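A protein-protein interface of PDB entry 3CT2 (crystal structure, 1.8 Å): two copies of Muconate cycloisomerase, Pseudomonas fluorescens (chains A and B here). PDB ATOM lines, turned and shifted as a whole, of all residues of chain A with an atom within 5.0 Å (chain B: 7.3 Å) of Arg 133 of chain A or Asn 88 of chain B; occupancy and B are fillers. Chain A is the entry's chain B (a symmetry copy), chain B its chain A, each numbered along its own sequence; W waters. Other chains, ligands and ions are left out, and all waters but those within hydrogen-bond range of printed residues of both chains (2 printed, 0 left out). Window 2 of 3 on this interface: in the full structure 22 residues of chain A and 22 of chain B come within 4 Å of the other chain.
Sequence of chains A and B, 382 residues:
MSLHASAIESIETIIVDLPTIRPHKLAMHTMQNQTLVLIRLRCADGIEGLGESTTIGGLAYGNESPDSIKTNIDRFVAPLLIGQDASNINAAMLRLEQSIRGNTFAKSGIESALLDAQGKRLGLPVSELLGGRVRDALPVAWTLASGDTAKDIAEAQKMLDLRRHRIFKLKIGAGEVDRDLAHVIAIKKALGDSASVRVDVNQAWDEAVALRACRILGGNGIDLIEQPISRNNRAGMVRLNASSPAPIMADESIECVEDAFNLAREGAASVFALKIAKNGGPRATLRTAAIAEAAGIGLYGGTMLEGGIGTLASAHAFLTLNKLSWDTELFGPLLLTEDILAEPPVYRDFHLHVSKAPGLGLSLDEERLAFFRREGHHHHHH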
ATOM      1  N   PRO A 125     -29.908  20.463   0.841  1.00  0.00           N
ATOM      2  CA  PRO A 125     -31.363  20.300   0.778  1.00  0.00           C
ATOM      3  C   PRO A 125     -31.933  20.584   2.169  1.00  0.00           C
ATOM      4  O   PRO A 125     -31.215  20.484   3.164  1.00  0.00           O
ATOM      5  CB  PRO A 125     -31.532  18.841   0.352  1.00  0.00           C
ATOM      6  CG  PRO A 125     -30.302  18.177   0.899  1.00  0.00           C
ATOM      7  CD  PRO A 125     -29.223  19.185   0.578  1.00  0.00           C
ATOM      8  N   SER A 127     -33.837  18.859   3.970  1.00  0.00           N
ATOM      9  CA  SER A 127     -33.735  17.675   4.805  1.00  0.00           C
ATOM     10  C   SER A 127     -32.410  17.646   5.566  1.00  0.00           C
ATOM     11  O   SER A 127     -32.354  17.162   6.696  1.00  0.00           O
ATOM     12  CB  SER A 127     -33.876  16.409   3.954  1.00  0.00           C
ATOM     13  OG  SER A 127     -32.872  16.353   2.963  1.00  0.00           O
ATOM     14  N   GLY A 131     -31.117  18.148   9.828  1.00  0.00           N
ATOM     15  CA  GLY A 131     -30.395  17.067  10.483  1.00  0.00           C
ATOM     16  C   GLY A 131     -29.887  15.946   9.599  1.00  0.00           C
ATOM     17  O   GLY A 131     -28.884  15.298   9.921  1.00  0.00           O
ATOM     18  N   GLY A 132     -30.568  15.705   8.487  1.00  0.00           N
ATOM     19  CA  GLY A 132     -30.140  14.645   7.593  1.00  0.00           C
ATOM     20  C   GLY A 132     -31.209  13.600   7.340  1.00  0.00           C
ATOM     21  O   GLY A 132     -31.870  13.117   8.264  1.00  0.00           O
ATOM     22  N   ARG A 133     -31.377  13.244   6.072  1.00  0.00           N
ATOM     23  CA  ARG A 133     -32.376  12.258   5.683  1.00  0.00           C
ATOM     24  C   ARG A 133     -31.921  10.838   5.997  1.00  0.00           C
ATOM     25  O   ARG A 133     -30.716  10.566   6.074  1.00  0.00           O
ATOM     26  CB  ARG A 133     -32.652  12.363   4.183  1.00  0.00           C
ATOM     27  CG  ARG A 133     -31.449  11.991   3.313  1.00  0.00           C
ATOM     28  CD  ARG A 133     -31.779  12.141   1.834  1.00  0.00           C
ATOM     29  NE  ARG A 133     -32.132  13.523   1.520  1.00  0.00           N
ATOM     30  CZ  ARG A 133     -32.780  13.901   0.424  1.00  0.00           C
ATOM     31  NH1 ARG A 133     -33.156  13.000  -0.479  1.00  0.00           N
ATOM     32  NH2 ARG A 133     -33.060  15.183   0.236  1.00  0.00           N
ATOM     33  N   VAL A 134     -32.887   9.941   6.184  1.00  0.00           N
ATOM     34  CA  VAL A 134     -32.600   8.530   6.437  1.00  0.00           C
ATOM     35  C   VAL A 134     -33.275   7.720   5.331  1.00  0.00           C
ATOM     36  O   VAL A 134     -33.237   6.489   5.322  1.00  0.00           O
ATOM     37  CB  VAL A 134     -33.119   8.059   7.824  1.00  0.00           C
ATOM     38  CG1 VAL A 134     -32.368   8.791   8.923  1.00  0.00           C
ATOM     39  CG2 VAL A 134     -34.614   8.299   7.948  1.00  0.00           C
ATOM     40  N   ARG A 135     -33.893   8.441   4.399  1.00  0.00           N
ATOM     41  CA  ARG A 135     -34.571   7.847   3.248  1.00  0.00           C
ATOM     42  C   ARG A 135     -34.671   8.917   2.161  1.00  0.00           C
ATOM     43  O   ARG A 135     -34.536  10.111   2.443  1.00  0.00           O
ATOM     44  CB  ARG A 135     -35.972   7.352   3.634  1.00  0.00           C
ATOM     45  CG  ARG A 135     -36.962   8.448   4.039  1.00  0.00           C
ATOM     46  CD  ARG A 135     -38.301   7.836   4.435  1.00  0.00           C
ATOM     47  NE  ARG A 135     -38.147   6.975   5.602  1.00  0.00           N
ATOM     48  CZ  ARG A 135     -38.024   7.421   6.850  1.00  0.00           C
ATOM     49  NH1 ARG A 135     -38.049   8.723   7.099  1.00  0.00           N
ATOM     50  NH2 ARG A 135     -37.846   6.564   7.847  1.00  0.00           N
ATOM     51  N   ASP A 136     -34.885   8.489   0.920  1.00  0.00           N
ATOM     52  CA  ASP A 136     -35.001   9.414  -0.205  1.00  0.00           C
ATOM     53  C   ASP A 136     -36.411   9.421  -0.779  1.00  0.00           C
ATOM     54  O   ASP A 136     -36.761  10.299  -1.573  1.00  0.00           O
ATOM     55  CB  ASP A 136     -34.030   9.018  -1.323  1.00  0.00           C
ATOM     56  CG  ASP A 136     -32.585   9.178  -0.922  1.00  0.00           C
ATOM     57  OD1 ASP A 136     -32.133  10.334  -0.768  1.00  0.00           O
ATOM     58  OD2 ASP A 136     -31.902   8.144  -0.757  1.00  0.00           O
ATOM     59  N   HIS A 316     -39.385  17.057   3.118  1.00  0.00           N
ATOM     60  CA  HIS A 316     -38.027  17.188   3.625  1.00  0.00           C
ATOM     61  C   HIS A 316     -37.951  16.950   5.124  1.00  0.00           C
ATOM     62  O   HIS A 316     -36.966  16.413   5.620  1.00  0.00           O
ATOM     63  CB  HIS A 316     -37.446  18.551   3.249  1.00  0.00           C
ATOM     64  CG  HIS A 316     -36.894  18.593   1.857  1.00  0.00           C
ATOM     65  ND1 HIS A 316     -35.548  18.476   1.588  1.00  0.00           N
ATOM     66  CD2 HIS A 316     -37.512  18.696   0.654  1.00  0.00           C
ATOM     67  CE1 HIS A 316     -35.358  18.507   0.279  1.00  0.00           C
ATOM     68  NE2 HIS A 316     -36.534  18.639  -0.310  1.00  0.00           N
ATOM     69  N   LEU A 319     -38.375  13.106   5.720  1.00  0.00           N
ATOM     70  CA  LEU A 319     -37.226  12.280   5.356  1.00  0.00           C
ATOM     71  C   LEU A 319     -36.290  12.046   6.545  1.00  0.00           C
ATOM     72  O   LEU A 319     -35.523  11.083   6.553  1.00  0.00           O
ATOM     73  CB  LEU A 319     -36.416  12.934   4.228  1.00  0.00           C
ATOM     74  CG  LEU A 319     -37.027  13.134   2.844  1.00  0.00           C
ATOM     75  CD1 LEU A 319     -35.939  13.655   1.903  1.00  0.00           C
ATOM     76  CD2 LEU A 319     -37.588  11.825   2.315  1.00  0.00           C
ATOM     77  N   THR A 320     -36.354  12.920   7.549  1.00  0.00           N
ATOM     78  CA  THR A 320     -35.476  12.806   8.713  1.00  0.00           C
ATOM     79  C   THR A 320     -36.004  11.924   9.840  1.00  0.00           C
ATOM     80  O   THR A 320     -35.270  11.612  10.783  1.00  0.00           O
ATOM     81  CB  THR A 320     -35.168  14.199   9.330  1.00  0.00           C
ATOM     82  OG1 THR A 320     -36.320  14.677  10.037  1.00  0.00           O
ATOM     83  CG2 THR A 320     -34.798  15.198   8.243  1.00  0.00           C
ATOM     84  N   VAL A 354     -37.805  12.395  -3.278  1.00  0.00           N
ATOM     85  CA  VAL A 354     -37.249  13.704  -2.972  1.00  0.00           C
ATOM     86  C   VAL A 354     -35.768  13.804  -3.310  1.00  0.00           C
ATOM     87  O   VAL A 354     -34.957  13.019  -2.827  1.00  0.00           O
ATOM     88  CB  VAL A 354     -37.449  14.036  -1.482  1.00  0.00           C
ATOM     89  CG1 VAL A 354     -37.041  15.477  -1.209  1.00  0.00           C
ATOM     90  CG2 VAL A 354     -38.906  13.803  -1.099  1.00  0.00           C
ATOM     91  N   SER A 355     -35.427  14.790  -4.136  1.00  0.00           N
ATOM     92  CA  SER A 355     -34.047  15.001  -4.565  1.00  0.00           C
ATOM     93  C   SER A 355     -33.183  15.602  -3.472  1.00  0.00           C
ATOM     94  O   SER A 355     -33.669  15.962  -2.392  1.00  0.00           O
ATOM     95  CB  SER A 355     -34.005  15.932  -5.776  1.00  0.00           C
ATOM     96  OG  SER A 355     -34.168  17.280  -5.366  1.00  0.00           O
ATOM     97  N   LYS A 356     -31.894  15.721  -3.769  1.00  0.00           N
ATOM     98  CA  LYS A 356     -30.940  16.288  -2.833  1.00  0.00           C
ATOM     99  C   LYS A 356     -30.549  17.694  -3.273  1.00  0.00           C
ATOM    100  O   LYS A 356     -29.517  18.212  -2.867  1.00  0.00           O
ATOM    101  CB  LYS A 356     -29.700  15.396  -2.744  1.00  0.00           C
ATOM    102  CG  LYS A 356     -30.030  13.957  -2.374  1.00  0.00           C
ATOM    103  CD  LYS A 356     -28.782  13.099  -2.204  1.00  0.00           C
ATOM    104  CE  LYS A 356     -29.164  11.660  -1.887  1.00  0.00           C
ATOM    105  NZ  LYS A 356     -27.977  10.782  -1.706  1.00  0.00           N
ATOM    106  N   SER B   6     -16.211  13.701   3.345  1.00  0.00           N
ATOM    107  CA  SER B   6     -16.881  13.513   4.629  1.00  0.00           C
ATOM    108  C   SER B   6     -16.852  12.137   5.283  1.00  0.00           C
ATOM    109  O   SER B   6     -17.247  12.004   6.439  1.00  0.00           O
ATOM    110  CB  SER B   6     -18.337  13.962   4.504  1.00  0.00           C
ATOM    111  OG  SER B   6     -18.397  15.320   4.120  1.00  0.00           O
ATOM    112  N   GLN B  84     -18.724   5.869   7.337  1.00  0.00           N
ATOM    113  CA  GLN B  84     -20.005   6.553   7.167  1.00  0.00           C
ATOM    114  C   GLN B  84     -19.806   8.045   6.897  1.00  0.00           C
ATOM    115  O   GLN B  84     -18.796   8.627   7.285  1.00  0.00           O
ATOM    116  CB  GLN B  84     -20.868   6.385   8.424  1.00  0.00           C
ATOM    117  CG  GLN B  84     -21.281   4.953   8.717  1.00  0.00           C
ATOM    118  CD  GLN B  84     -22.163   4.375   7.638  1.00  0.00           C
ATOM    119  OE1 GLN B  84     -23.244   4.902   7.354  1.00  0.00           O
ATOM    120  NE2 GLN B  84     -21.715   3.282   7.028  1.00  0.00           N
ATOM    121  N   ASP B  85     -20.778   8.660   6.235  1.00  0.00           N
ATOM    122  CA  ASP B  85     -20.715  10.084   5.924  1.00  0.00           C
ATOM    123  C   ASP B  85     -20.917  10.919   7.185  1.00  0.00           C
ATOM    124  O   ASP B  85     -22.013  10.961   7.750  1.00  0.00           O
ATOM    125  CB  ASP B  85     -21.778  10.424   4.877  1.00  0.00           C
ATOM    126  CG  ASP B  85     -21.893  11.913   4.620  1.00  0.00           C
ATOM    127  OD1 ASP B  85     -20.925  12.652   4.895  1.00  0.00           O
ATOM    128  OD2 ASP B  85     -22.957  12.342   4.131  1.00  0.00           O
ATOM    129  N   ALA B  86     -19.853  11.587   7.623  1.00  0.00           N
ATOM    130  CA  ALA B  86     -19.908  12.404   8.830  1.00  0.00           C
ATOM    131  C   ALA B  86     -20.818  13.625   8.716  1.00  0.00           C
ATOM    132  O   ALA B  86     -21.196  14.208   9.733  1.00  0.00           O
ATOM    133  CB  ALA B  86     -18.501  12.846   9.220  1.00  0.00           C
ATOM    134  N   SER B  87     -21.171  14.012   7.492  1.00  0.00           N
ATOM    135  CA  SER B  87     -22.021  15.181   7.288  1.00  0.00           C
ATOM    136  C   SER B  87     -23.512  14.930   7.531  1.00  0.00           C
ATOM    137  O   SER B  87     -24.300  15.877   7.590  1.00  0.00           O
ATOM    138  CB  SER B  87     -21.814  15.753   5.883  1.00  0.00           C
ATOM    139  OG  SER B  87     -22.228  14.837   4.888  1.00  0.00           O
ATOM    140  N   ASN B  88     -23.907  13.666   7.654  1.00  0.00           N
ATOM    141  CA  ASN B  88     -25.302  13.350   7.934  1.00  0.00           C
ATOM    142  C   ASN B  88     -25.327  12.825   9.364  1.00  0.00           C
ATOM    143  O   ASN B  88     -25.245  11.614   9.605  1.00  0.00           O
ATOM    144  CB  ASN B  88     -25.845  12.283   6.986  1.00  0.00           C
ATOM    145  CG  ASN B  88     -27.352  12.142   7.088  1.00  0.00           C
ATOM    146  OD1 ASN B  88     -27.929  12.321   8.162  1.00  0.00           O
ATOM    147  ND2 ASN B  88     -27.998  11.818   5.973  1.00  0.00           N
ATOM    148  N   ILE B  89     -25.443  13.746  10.309  1.00  0.00           N
ATOM    149  CA  ILE B  89     -25.429  13.392  11.719  1.00  0.00           C
ATOM    150  C   ILE B  89     -26.660  12.620  12.179  1.00  0.00           C
ATOM    151  O   ILE B  89     -26.548  11.697  12.987  1.00  0.00           O
ATOM    152  CB  ILE B  89     -25.228  14.658  12.576  1.00  0.00           C
ATOM    153  CG1 ILE B  89     -23.898  15.315  12.181  1.00  0.00           C
ATOM    154  CG2 ILE B  89     -25.250  14.301  14.066  1.00  0.00           C
ATOM    155  CD1 ILE B  89     -23.561  16.587  12.946  1.00  0.00           C
ATOM    156  N   ASN B  90     -27.829  12.976  11.662  1.00  0.00           N
ATOM    157  CA  ASN B  90     -29.052  12.275  12.047  1.00  0.00           C
ATOM    158  C   ASN B  90     -28.943  10.794  11.667  1.00  0.00           C
ATOM    159  O   ASN B  90     -29.256   9.913  12.468  1.00  0.00           O
ATOM    160  CB  ASN B  90     -30.267  12.911  11.361  1.00  0.00           C
ATOM    161  CG  ASN B  90     -31.574  12.263  11.772  1.00  0.00           C
ATOM    162  OD1 ASN B  90     -31.809  12.004  12.954  1.00  0.00           O
ATOM    163  ND2 ASN B  90     -32.441  12.011  10.799  1.00  0.00           N
ATOM    164  N   ALA B  91     -28.482  10.525  10.450  1.00  0.00           N
ATOM    165  CA  ALA B  91     -28.347   9.150   9.981  1.00  0.00           C
ATOM    166  C   ALA B  91     -27.322   8.378  10.805  1.00  0.00           C
ATOM    167  O   ALA B  91     -27.545   7.223  11.168  1.00  0.00           O
ATOM    168  CB  ALA B  91     -27.955   9.138   8.512  1.00  0.00           C
ATOM    169  N   ALA B  92     -26.197   9.018  11.103  1.00  0.00           N
ATOM    170  CA  ALA B  92     -25.145   8.376  11.883  1.00  0.00           C
ATOM    171  C   ALA B  92     -25.624   8.009  13.287  1.00  0.00           C
ATOM    172  O   ALA B  92     -25.371   6.904  13.773  1.00  0.00           O
ATOM    173  CB  ALA B  92     -23.923   9.295  11.977  1.00  0.00           C
ATOM    174  N   MET B  93     -26.319   8.934  13.941  1.00  0.00           N
ATOM    175  CA  MET B  93     -26.790   8.677  15.292  1.00  0.00           C
ATOM    176  C   MET B  93     -27.925   7.655  15.331  1.00  0.00           C
ATOM    177  O   MET B  93     -28.052   6.918  16.305  1.00  0.00           O
ATOM    178  CB  MET B  93     -27.191   9.990  15.972  1.00  0.00           C
ATOM    179  CG  MET B  93     -26.029  10.985  16.128  1.00  0.00           C
ATOM    180  SD  MET B  93     -24.538  10.349  16.994  1.00  0.00           S
ATOM    181  CE  MET B  93     -23.703   9.538  15.689  1.00  0.00           C
ATOM    182  N   LEU B  94     -28.735   7.592  14.276  1.00  0.00           N
ATOM    183  CA  LEU B  94     -29.818   6.612  14.231  1.00  0.00           C
ATOM    184  C   LEU B  94     -29.212   5.237  13.940  1.00  0.00           C
ATOM    185  O   LEU B  94     -29.731   4.210  14.385  1.00  0.00           O
ATOM    186  CB  LEU B  94     -30.842   6.982  13.152  1.00  0.00           C
ATOM    187  CG  LEU B  94     -31.758   8.157  13.515  1.00  0.00           C
ATOM    188  CD1 LEU B  94     -32.615   8.539  12.316  1.00  0.00           C
ATOM    189  CD2 LEU B  94     -32.640   7.775  14.709  1.00  0.00           C
ATOM    190  N   LEU B 114     -19.143  14.930  15.983  1.00  0.00           N
ATOM    191  CA  LEU B 114     -19.728  15.074  14.658  1.00  0.00           C
ATOM    192  C   LEU B 114     -20.203  16.503  14.416  1.00  0.00           C
ATOM    193  O   LEU B 114     -20.057  17.032  13.314  1.00  0.00           O
ATOM    194  CB  LEU B 114     -20.907  14.114  14.483  1.00  0.00           C
ATOM    195  CG  LEU B 114     -20.563  12.636  14.301  1.00  0.00           C
ATOM    196  CD1 LEU B 114     -21.837  11.815  14.384  1.00  0.00           C
ATOM    197  CD2 LEU B 114     -19.870  12.425  12.957  1.00  0.00           C
ATOM    198  N   GLN B 118     -18.815  19.027  11.604  1.00  0.00           N
ATOM    199  CA  GLN B 118     -19.732  19.569  10.612  1.00  0.00           C
ATOM    200  C   GLN B 118     -19.738  21.092  10.695  1.00  0.00           C
ATOM    201  O   GLN B 118     -19.904  21.773   9.686  1.00  0.00           O
ATOM    202  CB  GLN B 118     -21.144  19.014  10.830  1.00  0.00           C
ATOM    203  CG  GLN B 118     -22.173  19.412   9.765  1.00  0.00           C
ATOM    204  CD  GLN B 118     -21.743  19.063   8.347  1.00  0.00           C
ATOM    205  OE1 GLN B 118     -20.859  18.233   8.133  1.00  0.00           O
ATOM    206  NE2 GLN B 118     -22.380  19.694   7.366  1.00  0.00           N
ATOM    207  N   ARG B 283     -28.403  17.039  20.304  1.00  0.00           N
ATOM    208  CA  ARG B 283     -29.650  16.881  19.562  1.00  0.00           C
ATOM    209  C   ARG B 283     -30.736  16.176  20.373  1.00  0.00           C
ATOM    210  O   ARG B 283     -31.878  16.637  20.418  1.00  0.00           O
ATOM    211  CB  ARG B 283     -29.383  16.152  18.241  1.00  0.00           C
ATOM    212  CG  ARG B 283     -28.496  16.980  17.307  1.00  0.00           C
ATOM    213  CD  ARG B 283     -28.103  16.242  16.027  1.00  0.00           C
ATOM    214  NE  ARG B 283     -29.261  15.831  15.241  1.00  0.00           N
ATOM    215  CZ  ARG B 283     -29.708  14.580  15.171  1.00  0.00           C
ATOM    216  NH1 ARG B 283     -29.088  13.612  15.839  1.00  0.00           N
ATOM    217  NH2 ARG B 283     -30.776  14.297  14.436  1.00  0.00           N
HETATM  218  O   HOH W   1     -34.528  11.974  13.973  1.00  0.00           O
HETATM  219  O   HOH W   2     -26.499  16.665   9.905  1.00  0.00           O
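Of the printed residues of chain B, Gly 132 of chain A touches Asn 88 and Asn 90. Of the printed residues of chain B, Val 134 of chain A touches Asn 90 (3.7 Å) and Leu 94 (3.4 Å). Asn 88 of chain B touches just these residues of chain A: Gly 131 (3.6 Å), Gly 132 (3.3 Å) and Arg 133 (3.0 Å). Printed residues of chain A within 4 Å of Ala 91 of chain B: Arg 133 (3.95 Å). The nearest residue of chain B that does not touch Arg 133 of chain A is Asn 90 of chain B (5.0 Å).
Water W2 lies within hydrogen-bond range of the backbone carbonyl oxygen of Gly 131 of chain A, the backbone NH of Ile 89 of chain B and the backbone carbonyl oxygen of Ser 87 of chain B. Water W1 lies within hydrogen-bond range of OD1 of Asn 90 of chain B and O of Thr 320 of chain A.
No position is printed for both chains.
O of Thr 320 of chain A sits at hydrogen-bond distance from ND2 of Asn 90 of chain B (2.9 Å). O of Gly 131 of chain A lies within hydrogen-bond range of N of Asn 90 of chain B (3.1 Å). The side-chain amide nitrogen of Asn 90 of chain B is in hydrogen-bond range of the backbone carbonyl oxygen of Gly 132 of chain A (2.8 Å). ND2 of Asn 88 of chain B sits at hydrogen-bond distance from O of Arg 133 of chain A.
Among the printed residues, pairs that only touch across the chains: Gly 132 of chain A with Asn 88 of chain B, Val 134 of chain A with Leu 94 of chain B, Gly 131 of chain A with Asn 88 of chain B, Val 134 of chain A with Asn 90 of chain B, Gly 131 of chain A with Ile 89 of chain B and Arg 133 of chain A with Ala 91 of chain B.
OD1 of Asn 88 of chain B sits at hydrogen-bond distance from N of Ala 91 of chain B, at 3.0 Å. NH1 of Arg 133 of chain A is in hydrogen-bond range of O of Val 354 of chain A, 3.0 Å away. OD1 of Asn 90 of chain B lies within hydrogen-bond range of NH2 of Arg 283 of chain B, 2.9 Å away. The backbone carbonyl oxygen (O) of Ser 127 of chain A sits at hydrogen-bond distance from the backbone NH (N) of Gly 132 of chain A (2.9 Å). O of Leu 319 of chain A is in hydrogen-bond range of N of Val 134 of chain A (2.9 Å). OG of Ser 127 of chain A is in hydrogen-bond range of NH2 of Arg 133 of chain A.
Hydrophobic or aromatic side chains of chain B that line the printed part of chain A: Ala 91 and Leu 94. Printed residues of chain A that touch a printed residue of chain B: Gly 131, Gly 132, Arg 133, Val 134 and Thr 320.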
